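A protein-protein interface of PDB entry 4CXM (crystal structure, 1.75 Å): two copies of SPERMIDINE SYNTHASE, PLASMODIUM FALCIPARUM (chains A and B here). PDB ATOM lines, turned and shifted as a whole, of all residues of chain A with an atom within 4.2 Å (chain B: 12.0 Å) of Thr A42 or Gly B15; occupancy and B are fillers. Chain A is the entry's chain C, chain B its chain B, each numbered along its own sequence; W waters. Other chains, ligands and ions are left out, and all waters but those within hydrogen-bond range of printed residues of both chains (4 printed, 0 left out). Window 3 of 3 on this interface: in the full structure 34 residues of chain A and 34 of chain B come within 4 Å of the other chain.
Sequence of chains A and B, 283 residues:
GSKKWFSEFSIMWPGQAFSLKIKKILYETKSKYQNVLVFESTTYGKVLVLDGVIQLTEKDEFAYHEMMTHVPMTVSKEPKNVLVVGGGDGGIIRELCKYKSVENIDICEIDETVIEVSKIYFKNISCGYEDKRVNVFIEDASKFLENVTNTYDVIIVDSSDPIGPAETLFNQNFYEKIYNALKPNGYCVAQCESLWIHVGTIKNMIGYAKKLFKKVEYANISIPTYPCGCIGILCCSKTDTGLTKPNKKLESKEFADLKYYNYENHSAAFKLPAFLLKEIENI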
ATOM      1  N   LYS A   3     -10.623 -34.331  19.368  1.00  0.00           N
ATOM      2  CA  LYS A   3     -11.969 -35.064  19.336  1.00  0.00           C
ATOM      3  C   LYS A   3     -12.625 -35.035  17.969  1.00  0.00           C
ATOM      4  O   LYS A   3     -12.804 -34.011  17.382  1.00  0.00           O
ATOM      5  CB  LYS A   3     -12.978 -34.580  20.379  1.00  0.00           C
ATOM      6  CG  LYS A   3     -12.885 -35.389  21.663  1.00  0.00           C
ATOM      7  CD  LYS A   3     -13.891 -34.928  22.689  1.00  0.00           C
ATOM      8  CE  LYS A   3     -13.627 -35.582  24.017  1.00  0.00           C
ATOM      9  NZ  LYS A   3     -14.448 -34.893  25.050  1.00  0.00           N
ATOM     10  N   TRP A   5     -15.589 -36.156  15.128  1.00  0.00           N
ATOM     11  CA  TRP A   5     -17.046 -36.106  15.022  1.00  0.00           C
ATOM     12  C   TRP A   5     -17.542 -37.282  14.228  1.00  0.00           C
ATOM     13  O   TRP A   5     -16.929 -37.733  13.250  1.00  0.00           O
ATOM     14  CB  TRP A   5     -17.483 -34.824  14.379  1.00  0.00           C
ATOM     15  CG  TRP A   5     -17.288 -33.608  15.197  1.00  0.00           C
ATOM     16  CD1 TRP A   5     -16.062 -32.993  15.505  1.00  0.00           C
ATOM     17  CD2 TRP A   5     -18.288 -32.799  15.824  1.00  0.00           C
ATOM     18  NE1 TRP A   5     -16.270 -31.867  16.245  1.00  0.00           N
ATOM     19  CE2 TRP A   5     -17.617 -31.715  16.470  1.00  0.00           C
ATOM     20  CE3 TRP A   5     -19.664 -32.864  15.902  1.00  0.00           C
ATOM     21  CZ2 TRP A   5     -18.299 -30.716  17.182  1.00  0.00           C
ATOM     22  CZ3 TRP A   5     -20.334 -31.829  16.594  1.00  0.00           C
ATOM     23  CH2 TRP A   5     -19.680 -30.813  17.216  1.00  0.00           C
ATOM     24  N   SER A  19     -24.396 -34.185  12.913  1.00  0.00           N
ATOM     25  CA  SER A  19     -23.117 -34.726  13.505  1.00  0.00           C
ATOM     26  C   SER A  19     -23.159 -34.638  15.005  1.00  0.00           C
ATOM     27  O   SER A  19     -23.720 -33.744  15.645  1.00  0.00           O
ATOM     28  CB  SER A  19     -21.933 -33.890  12.992  1.00  0.00           C
ATOM     29  OG  SER A  19     -21.798 -33.865  11.604  1.00  0.00           O
ATOM     30  N   LEU A  20     -22.414 -35.552  15.646  1.00  0.00           N
ATOM     31  CA  LEU A  20     -22.301 -35.609  17.084  1.00  0.00           C
ATOM     32  C   LEU A  20     -20.769 -35.791  17.412  1.00  0.00           C
ATOM     33  O   LEU A  20     -20.087 -36.514  16.714  1.00  0.00           O
ATOM     34  CB  LEU A  20     -23.051 -36.789  17.705  1.00  0.00           C
ATOM     35  CG  LEU A  20     -24.576 -36.829  17.603  1.00  0.00           C
ATOM     36  CD1 LEU A  20     -25.062 -38.201  17.944  1.00  0.00           C
ATOM     37  CD2 LEU A  20     -25.042 -35.723  18.562  1.00  0.00           C
ATOM     38  N   LYS A  21     -20.361 -35.027  18.379  1.00  0.00           N
ATOM     39  CA  LYS A  21     -18.974 -35.102  18.904  1.00  0.00           C
ATOM     40  C   LYS A  21     -18.782 -36.376  19.694  1.00  0.00           C
ATOM     41  O   LYS A  21     -19.596 -36.754  20.525  1.00  0.00           O
ATOM     42  CB  LYS A  21     -18.640 -33.839  19.675  1.00  0.00           C
ATOM     43  CG  LYS A  21     -17.210 -33.778  20.195  1.00  0.00           C
ATOM     44  CD  LYS A  21     -16.910 -32.471  20.852  1.00  0.00           C
ATOM     45  CE  LYS A  21     -16.463 -31.446  19.880  1.00  0.00           C
ATOM     46  NZ  LYS A  21     -16.110 -30.196  20.630  1.00  0.00           N
ATOM     47  N   LYS A  23     -16.965 -38.754  22.227  1.00  0.00           N
ATOM     48  CA  LYS A  23     -16.136 -38.870  23.388  1.00  0.00           C
ATOM     49  C   LYS A  23     -15.227 -40.065  23.236  1.00  0.00           C
ATOM     50  O   LYS A  23     -13.987 -39.925  23.348  1.00  0.00           O
ATOM     51  CB  LYS A  23     -16.957 -39.013  24.621  1.00  0.00           C
ATOM     52  CG  LYS A  23     -16.112 -38.907  25.914  1.00  0.00           C
ATOM     53  CD  LYS A  23     -17.072 -38.881  27.074  1.00  0.00           C
ATOM     54  CE  LYS A  23     -17.691 -37.491  27.295  1.00  0.00           C
ATOM     55  NZ  LYS A  23     -18.515 -37.470  28.548  1.00  0.00           N
ATOM     56  N   SER A  41     -21.162 -40.292  22.825  1.00  0.00           N
ATOM     57  CA  SER A  41     -21.129 -38.892  22.396  1.00  0.00           C
ATOM     58  C   SER A  41     -20.840 -38.014  23.601  1.00  0.00           C
ATOM     59  O   SER A  41     -21.025 -38.403  24.722  1.00  0.00           O
ATOM     60  CB  SER A  41     -22.452 -38.514  21.656  1.00  0.00           C
ATOM     61  OG  SER A  41     -23.411 -38.361  22.644  1.00  0.00           O
ATOM     62  N   THR A  42     -20.493 -36.757  23.362  1.00  0.00           N
ATOM     63  CA  THR A  42     -20.261 -35.837  24.438  1.00  0.00           C
ATOM     64  C   THR A  42     -21.522 -35.303  25.043  1.00  0.00           C
ATOM     65  O   THR A  42     -21.525 -35.026  26.179  1.00  0.00           O
ATOM     66  CB  THR A  42     -19.398 -34.635  24.034  1.00  0.00           C
ATOM     67  OG1 THR A  42     -20.096 -33.905  23.004  1.00  0.00           O
ATOM     68  CG2 THR A  42     -18.056 -35.098  23.562  1.00  0.00           C
ATOM     69  N   THR A  43     -22.656 -35.244  24.318  1.00  0.00           N
ATOM     70  CA  THR A  43     -23.849 -34.670  24.939  1.00  0.00           C
ATOM     71  C   THR A  43     -25.169 -35.456  24.860  1.00  0.00           C
ATOM     72  O   THR A  43     -26.100 -35.106  25.520  1.00  0.00           O
ATOM     73  CB  THR A  43     -24.080 -33.225  24.438  1.00  0.00           C
ATOM     74  OG1 THR A  43     -24.390 -33.243  23.057  1.00  0.00           O
ATOM     75  CG2 THR A  43     -22.818 -32.390  24.664  1.00  0.00           C
ATOM     76  N   TYR A  44     -25.179 -36.568  24.178  1.00  0.00           N
ATOM     77  CA  TYR A  44     -26.354 -37.421  24.028  1.00  0.00           C
ATOM     78  C   TYR A  44     -26.170 -38.797  24.638  1.00  0.00           C
ATOM     79  O   TYR A  44     -26.970 -39.706  24.484  1.00  0.00           O
ATOM     80  CB  TYR A  44     -26.772 -37.536  22.544  1.00  0.00           C
ATOM     81  CG  TYR A  44     -27.452 -36.272  21.996  1.00  0.00           C
ATOM     82  CD1 TYR A  44     -26.718 -35.163  21.639  1.00  0.00           C
ATOM     83  CD2 TYR A  44     -28.863 -36.221  21.809  1.00  0.00           C
ATOM     84  CE1 TYR A  44     -27.333 -34.017  21.129  1.00  0.00           C
ATOM     85  CE2 TYR A  44     -29.485 -35.065  21.339  1.00  0.00           C
ATOM     86  CZ  TYR A  44     -28.727 -33.989  20.993  1.00  0.00           C
ATOM     87  OH  TYR A  44     -29.341 -32.845  20.495  1.00  0.00           O
ATOM     88  N   SER B   7     -21.563 -25.803   7.797  1.00  0.00           N
ATOM     89  CA  SER B   7     -21.798 -26.420   9.074  1.00  0.00           C
ATOM     90  C   SER B   7     -22.130 -25.416  10.142  1.00  0.00           C
ATOM     91  O   SER B   7     -21.445 -24.386  10.317  1.00  0.00           O
ATOM     92  CB  SER B   7     -20.570 -27.244   9.508  1.00  0.00           C
ATOM     93  OG  SER B   7     -20.416 -28.381   8.677  1.00  0.00           O
ATOM     94  N   GLU B   8     -23.162 -25.707  10.921  1.00  0.00           N
ATOM     95  CA  GLU B   8     -23.613 -24.792  11.948  1.00  0.00           C
ATOM     96  C   GLU B   8     -23.189 -25.422  13.265  1.00  0.00           C
ATOM     97  O   GLU B   8     -23.712 -26.467  13.628  1.00  0.00           O
ATOM     98  CB  GLU B   8     -25.140 -24.661  11.937  1.00  0.00           C
ATOM     99  CG  GLU B   8     -25.701 -23.733  13.002  1.00  0.00           C
ATOM    100  CD  GLU B   8     -27.205 -23.795  13.137  1.00  0.00           C
ATOM    101  OE1 GLU B   8     -27.647 -24.926  13.458  1.00  0.00           O
ATOM    102  OE2 GLU B   8     -27.910 -22.738  13.006  1.00  0.00           O
ATOM    103  N   PHE B   9     -22.217 -24.825  13.939  1.00  0.00           N
ATOM    104  CA  PHE B   9     -21.590 -25.304  15.209  1.00  0.00           C
ATOM    105  C   PHE B   9     -21.803 -24.099  16.080  1.00  0.00           C
ATOM    106  O   PHE B   9     -21.593 -23.010  15.592  1.00  0.00           O
ATOM    107  CB  PHE B   9     -20.023 -25.406  15.098  1.00  0.00           C
ATOM    108  CG  PHE B   9     -19.496 -26.487  14.253  1.00  0.00           C
ATOM    109  CD1 PHE B   9     -19.329 -27.815  14.787  1.00  0.00           C
ATOM    110  CD2 PHE B   9     -19.009 -26.217  12.983  1.00  0.00           C
ATOM    111  CE1 PHE B   9     -18.756 -28.869  14.032  1.00  0.00           C
ATOM    112  CE2 PHE B   9     -18.447 -27.275  12.213  1.00  0.00           C
ATOM    113  CZ  PHE B   9     -18.319 -28.599  12.740  1.00  0.00           C
ATOM    114  N   SER B  10     -22.095 -24.271  17.350  1.00  0.00           N
ATOM    115  CA  SER B  10     -22.226 -23.215  18.285  1.00  0.00           C
ATOM    116  C   SER B  10     -21.961 -23.581  19.751  1.00  0.00           C
ATOM    117  O   SER B  10     -22.324 -24.667  20.241  1.00  0.00           O
ATOM    118  CB  SER B  10     -23.635 -22.602  18.148  1.00  0.00           C
ATOM    119  OG  SER B  10     -23.785 -21.593  19.065  1.00  0.00           O
ATOM    120  N   ILE B  11     -21.380 -22.607  20.487  1.00  0.00           N
ATOM    121  CA  ILE B  11     -21.319 -22.654  21.927  1.00  0.00           C
ATOM    122  C   ILE B  11     -22.673 -22.734  22.570  1.00  0.00           C
ATOM    123  O   ILE B  11     -22.778 -23.201  23.667  1.00  0.00           O
ATOM    124  CB  ILE B  11     -20.445 -21.490  22.519  1.00  0.00           C
ATOM    125  CG1 ILE B  11     -21.053 -20.105  22.381  1.00  0.00           C
ATOM    126  CG2 ILE B  11     -19.039 -21.549  21.829  1.00  0.00           C
ATOM    127  CD1 ILE B  11     -20.182 -19.085  23.157  1.00  0.00           C
ATOM    128  N   MET B  12     -23.739 -22.350  21.856  1.00  0.00           N
ATOM    129  CA  MET B  12     -25.118 -22.434  22.417  1.00  0.00           C
ATOM    130  C   MET B  12     -25.696 -23.878  22.424  1.00  0.00           C
ATOM    131  O   MET B  12     -26.703 -24.198  23.116  1.00  0.00           O
ATOM    132  CB  MET B  12     -26.001 -21.470  21.597  1.00  0.00           C
ATOM    133  CG  MET B  12     -25.712 -19.997  21.891  1.00  0.00           C
ATOM    134  SD  MET B  12     -26.710 -18.767  20.985  1.00  0.00           S
ATOM    135  CE  MET B  12     -26.284 -19.113  19.298  1.00  0.00           C
ATOM    136  N   TRP B  13     -25.093 -24.752  21.617  1.00  0.00           N
ATOM    137  CA  TRP B  13     -25.491 -26.148  21.513  1.00  0.00           C
ATOM    138  C   TRP B  13     -24.249 -27.074  21.248  1.00  0.00           C
ATOM    139  O   TRP B  13     -24.054 -27.658  20.202  1.00  0.00           O
ATOM    140  CB  TRP B  13     -26.581 -26.374  20.470  1.00  0.00           C
ATOM    141  CG  TRP B  13     -26.419 -25.689  19.137  1.00  0.00           C
ATOM    142  CD1 TRP B  13     -25.798 -26.162  18.103  1.00  0.00           C
ATOM    143  CD2 TRP B  13     -26.954 -24.418  18.758  1.00  0.00           C
ATOM    144  NE1 TRP B  13     -25.810 -25.290  17.076  1.00  0.00           N
ATOM    145  CE2 TRP B  13     -26.587 -24.210  17.438  1.00  0.00           C
ATOM    146  CE3 TRP B  13     -27.753 -23.489  19.393  1.00  0.00           C
ATOM    147  CZ2 TRP B  13     -26.945 -23.066  16.715  1.00  0.00           C
ATOM    148  CZ3 TRP B  13     -28.124 -22.299  18.696  1.00  0.00           C
ATOM    149  CH2 TRP B  13     -27.666 -22.109  17.358  1.00  0.00           C
ATOM    150  N   PRO B  14     -23.435 -27.224  22.273  1.00  0.00           N
ATOM    151  CA  PRO B  14     -22.166 -27.870  22.014  1.00  0.00           C
ATOM    152  C   PRO B  14     -22.364 -29.354  21.835  1.00  0.00           C
ATOM    153  O   PRO B  14     -23.345 -29.970  22.352  1.00  0.00           O
ATOM    154  CB  PRO B  14     -21.347 -27.601  23.319  1.00  0.00           C
ATOM    155  CG  PRO B  14     -22.314 -27.122  24.323  1.00  0.00           C
ATOM    156  CD  PRO B  14     -23.508 -26.604  23.603  1.00  0.00           C
ATOM    157  N   GLY B  15     -21.452 -29.944  21.099  1.00  0.00           N
ATOM    158  CA  GLY B  15     -21.476 -31.400  20.922  1.00  0.00           C
ATOM    159  C   GLY B  15     -22.281 -31.903  19.735  1.00  0.00           C
ATOM    160  O   GLY B  15     -22.352 -33.097  19.507  1.00  0.00           O
ATOM    161  N   GLN B  16     -22.977 -31.007  19.028  1.00  0.00           N
ATOM    162  CA  GLN B  16     -23.778 -31.379  17.872  1.00  0.00           C
ATOM    163  C   GLN B  16     -23.599 -30.342  16.784  1.00  0.00           C
ATOM    164  O   GLN B  16     -23.218 -29.178  17.039  1.00  0.00           O
ATOM    165  CB  GLN B  16     -25.244 -31.446  18.261  1.00  0.00           C
ATOM    166  CG  GLN B  16     -25.818 -30.093  18.603  1.00  0.00           C
ATOM    167  CD  GLN B  16     -27.259 -30.297  19.133  1.00  0.00           C
ATOM    168  OE1 GLN B  16     -27.482 -30.866  20.199  1.00  0.00           O
ATOM    169  NE2 GLN B  16     -28.244 -29.895  18.321  1.00  0.00           N
ATOM    170  N   ALA B  17     -23.958 -30.704  15.590  1.00  0.00           N
ATOM    171  CA  ALA B  17     -23.866 -29.775  14.442  1.00  0.00           C
ATOM    172  C   ALA B  17     -24.764 -30.237  13.348  1.00  0.00           C
ATOM    173  O   ALA B  17     -25.048 -31.400  13.211  1.00  0.00           O
ATOM    174  CB  ALA B  17     -22.426 -29.694  13.902  1.00  0.00           C
ATOM    175  N   PHE B  18     -25.228 -29.318  12.535  1.00  0.00           N
ATOM    176  CA  PHE B  18     -26.022 -29.602  11.372  1.00  0.00           C
ATOM    177  C   PHE B  18     -25.366 -28.961  10.148  1.00  0.00           C
ATOM    178  O   PHE B  18     -24.881 -27.826  10.217  1.00  0.00           O
ATOM    179  CB  PHE B  18     -27.469 -29.022  11.559  1.00  0.00           C
ATOM    180  CG  PHE B  18     -28.359 -29.247  10.402  1.00  0.00           C
ATOM    181  CD1 PHE B  18     -28.801 -30.507  10.042  1.00  0.00           C
ATOM    182  CD2 PHE B  18     -28.803 -28.183   9.688  1.00  0.00           C
ATOM    183  CE1 PHE B  18     -29.671 -30.688   8.983  1.00  0.00           C
ATOM    184  CE2 PHE B  18     -29.626 -28.375   8.577  1.00  0.00           C
ATOM    185  CZ  PHE B  18     -30.099 -29.601   8.241  1.00  0.00           C
ATOM    186  N   SER B  19     -25.270 -29.726   9.096  1.00  0.00           N
ATOM    187  CA  SER B  19     -24.657 -29.314   7.873  1.00  0.00           C
ATOM    188  C   SER B  19     -25.631 -29.360   6.668  1.00  0.00           C
ATOM    189  O   SER B  19     -26.453 -30.273   6.544  1.00  0.00           O
ATOM    190  CB  SER B  19     -23.398 -30.162   7.556  1.00  0.00           C
ATOM    191  OG  SER B  19     -22.528 -29.992   8.614  1.00  0.00           O
ATOM    192  N   GLU B 193     -35.998 -20.991  23.315  1.00  0.00           N
ATOM    193  CA  GLU B 193     -35.111 -22.106  23.214  1.00  0.00           C
ATOM    194  C   GLU B 193     -35.825 -23.422  22.945  1.00  0.00           C
ATOM    195  O   GLU B 193     -36.887 -23.656  23.567  1.00  0.00           O
ATOM    196  CB  GLU B 193     -34.534 -22.198  24.595  1.00  0.00           C
ATOM    197  CG  GLU B 193     -33.420 -23.282  24.661  1.00  0.00           C
ATOM    198  CD  GLU B 193     -32.056 -22.842  24.103  1.00  0.00           C
ATOM    199  OE1 GLU B 193     -31.908 -21.640  23.691  1.00  0.00           O
ATOM    200  OE2 GLU B 193     -31.104 -23.720  24.196  1.00  0.00           O
ATOM    201  N   TRP B 196     -35.238 -29.456  23.616  1.00  0.00           N
ATOM    202  CA  TRP B 196     -34.206 -30.513  23.611  1.00  0.00           C
ATOM    203  C   TRP B 196     -32.818 -30.005  23.993  1.00  0.00           C
ATOM    204  O   TRP B 196     -32.001 -30.810  24.219  1.00  0.00           O
ATOM    205  CB  TRP B 196     -34.186 -31.226  22.299  1.00  0.00           C
ATOM    206  CG  TRP B 196     -35.338 -32.132  22.014  1.00  0.00           C
ATOM    207  CD1 TRP B 196     -36.374 -31.879  21.144  1.00  0.00           C
ATOM    208  CD2 TRP B 196     -35.630 -33.378  22.614  1.00  0.00           C
ATOM    209  NE1 TRP B 196     -37.218 -32.915  21.143  1.00  0.00           N
ATOM    210  CE2 TRP B 196     -36.840 -33.838  22.061  1.00  0.00           C
ATOM    211  CE3 TRP B 196     -35.003 -34.161  23.576  1.00  0.00           C
ATOM    212  CZ2 TRP B 196     -37.413 -35.074  22.414  1.00  0.00           C
ATOM    213  CZ3 TRP B 196     -35.535 -35.381  23.927  1.00  0.00           C
ATOM    214  CH2 TRP B 196     -36.741 -35.841  23.354  1.00  0.00           C
ATOM    215  N   ILE B 197     -32.631 -28.699  24.182  1.00  0.00           N
ATOM    216  CA  ILE B 197     -31.309 -28.083  24.423  1.00  0.00           C
ATOM    217  C   ILE B 197     -31.296 -27.497  25.861  1.00  0.00           C
ATOM    218  O   ILE B 197     -31.020 -28.240  26.767  1.00  0.00           O
ATOM    219  CB  ILE B 197     -30.999 -26.965  23.378  1.00  0.00           C
ATOM    220  CG1 ILE B 197     -31.154 -27.479  21.975  1.00  0.00           C
ATOM    221  CG2 ILE B 197     -29.549 -26.453  23.590  1.00  0.00           C
ATOM    222  CD1 ILE B 197     -30.760 -26.491  20.886  1.00  0.00           C
ATOM    223  N   HIS B 198     -31.725 -26.272  26.119  1.00  0.00           N
ATOM    224  CA  HIS B 198     -31.594 -25.672  27.501  1.00  0.00           C
ATOM    225  C   HIS B 198     -32.929 -25.359  28.066  1.00  0.00           C
ATOM    226  O   HIS B 198     -33.503 -24.232  27.885  1.00  0.00           O
ATOM    227  CB  HIS B 198     -30.675 -24.437  27.589  1.00  0.00           C
ATOM    228  CG  HIS B 198     -29.289 -24.712  27.150  1.00  0.00           C
ATOM    229  ND1 HIS B 198     -28.570 -23.861  26.332  1.00  0.00           N
ATOM    230  CD2 HIS B 198     -28.513 -25.795  27.352  1.00  0.00           C
ATOM    231  CE1 HIS B 198     -27.402 -24.414  26.049  1.00  0.00           C
ATOM    232  NE2 HIS B 198     -27.347 -25.589  26.649  1.00  0.00           N
ATOM    233  N   PRO B 227     -31.467 -25.936  15.396  1.00  0.00           N
ATOM    234  CA  PRO B 227     -30.863 -27.019  16.140  1.00  0.00           C
ATOM    235  C   PRO B 227     -31.850 -27.892  16.890  1.00  0.00           C
ATOM    236  O   PRO B 227     -32.756 -27.326  17.501  1.00  0.00           O
ATOM    237  CB  PRO B 227     -29.985 -26.265  17.158  1.00  0.00           C
ATOM    238  CG  PRO B 227     -30.059 -24.850  16.914  1.00  0.00           C
ATOM    239  CD  PRO B 227     -30.991 -24.604  15.799  1.00  0.00           C
ATOM    240  N   CYS B 228     -31.730 -29.211  16.799  1.00  0.00           N
ATOM    241  CA  CYS B 228     -32.641 -30.189  17.408  1.00  0.00           C
ATOM    242  C   CYS B 228     -33.983 -30.325  16.649  1.00  0.00           C
ATOM    243  O   CYS B 228     -34.828 -31.085  17.068  1.00  0.00           O
ATOM    244  CB  CYS B 228     -32.878 -29.952  18.875  1.00  0.00           C
ATOM    245  SG  CYS B 228     -31.324 -30.278  19.854  1.00  0.00           S
HETATM  246  O   HOH W   1     -23.227 -31.908  10.562  1.00  0.00           O
HETATM  247  O   HOH W   2     -22.764 -35.113  21.379  1.00  0.00           O
HETATM  248  O   HOH W   3     -18.845 -28.736  20.559  1.00  0.00           O
HETATM  249  O   HOH W   4     -26.140 -31.201  22.419  1.00  0.00           O
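Water W4 lies within hydrogen-bond range of the side-chain amide oxygen (OE1) of Gln B16, the side-chain hydroxyl (OG1) of Thr A43 and the backbone carbonyl oxygen (O) of Pro B14.
Water W1 lies within hydrogen-bond range of the side-chain hydroxyl (OG) of Ser A19 (2.6 Å), the side-chain hydroxyl (OG) of Ser B19 (2.8 Å) and the backbone carbonyl oxygen (O) of Ala B17 (3.3 Å).
Water W2 lies within hydrogen-bond range of the backbone carbonyl oxygen of Gly B15 (2.8 Å), the backbone NH of Thr A43 (2.9 Å) and the side-chain hydroxyl of Thr A42 (3.3 Å).
Water W3 lies within hydrogen-bond range of the backbone NH of Gly B15 and the side-chain amino group of Lys A21.
The backbone carbonyl oxygen of Lys A21 sits at hydrogen-bond distance from the backbone NH of Thr A42 (3.0 Å).
The backbone NH (N) of Tyr A44 sits at hydrogen-bond distance from the side-chain hydroxyl (OG) of Ser A41 (2.9 Å).
The side-chain sulfur of Cys B228 is in hydrogen-bond range of the side-chain amide nitrogen of Gln B16, 3.5 Å away.
Hydrophobic or aromatic side chains of chain A within 4 Å of the printed part of chain B: Trp A5, Leu A20 and Tyr A44.
Of chain A, only Trp A5, Leu A20, Lys A21 and Thr A42 come within 4 Å of Gly B15.
Leu A20 touches just one residue of chain B: Gly B15.
Lys A21 touches just one residue of chain B: Gly B15.
Of chain B, only Pro B14 (3.4 Å) comes within 4 Å of Thr A43.
Printed residues of chain A within 4 Å of Phe B9: Trp A5.
Of the printed residues of chain A, Pro B14 touches Thr A43 (3.4 Å).
The nearest residue of chain A that does not touch Gly B15 is Thr A43 (4.1 Å).
The nearest printed residue of chain A that does not touch Pro B14 is Thr A42 (5.1 Å).
O of Ala B17 is in hydrogen-bond range of N of Ser A19.
The backbone carbonyl oxygen (O) of Gly B15 is in hydrogen-bond range of the backbone NH (N) of Lys A21 (3.0 Å).
The side-chain amide oxygen of Gln B16 lies within hydrogen-bond range of the side-chain hydroxyl of Tyr A44 (2.7 Å).
SG of Cys B228 sits at hydrogen-bond distance from OH of Tyr A44, 3.3 Å away.
Phe B9 touches Trp A5.
Gly B15 touches Trp A5.
C of Gln B16 touches CZ3 of Trp A5, at 3.6 Å.
Trp A5 touches Ala B17 (CZ3 to N, 3.9 Å).
Ser A19 touches Gln B16 (O to CA, 3.2 Å).
O of Gly B15 touches CA of Leu A20, at 3.5 Å.
Gly B15 touches Thr A42 (CA to OG1, 3.5 Å).
Thr A43 touches Pro B14.
1 position is printed for both chains.
Of the 12 pairs that touch across the chains among the printed residues, none has its exchanged pair printed and touching as well.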
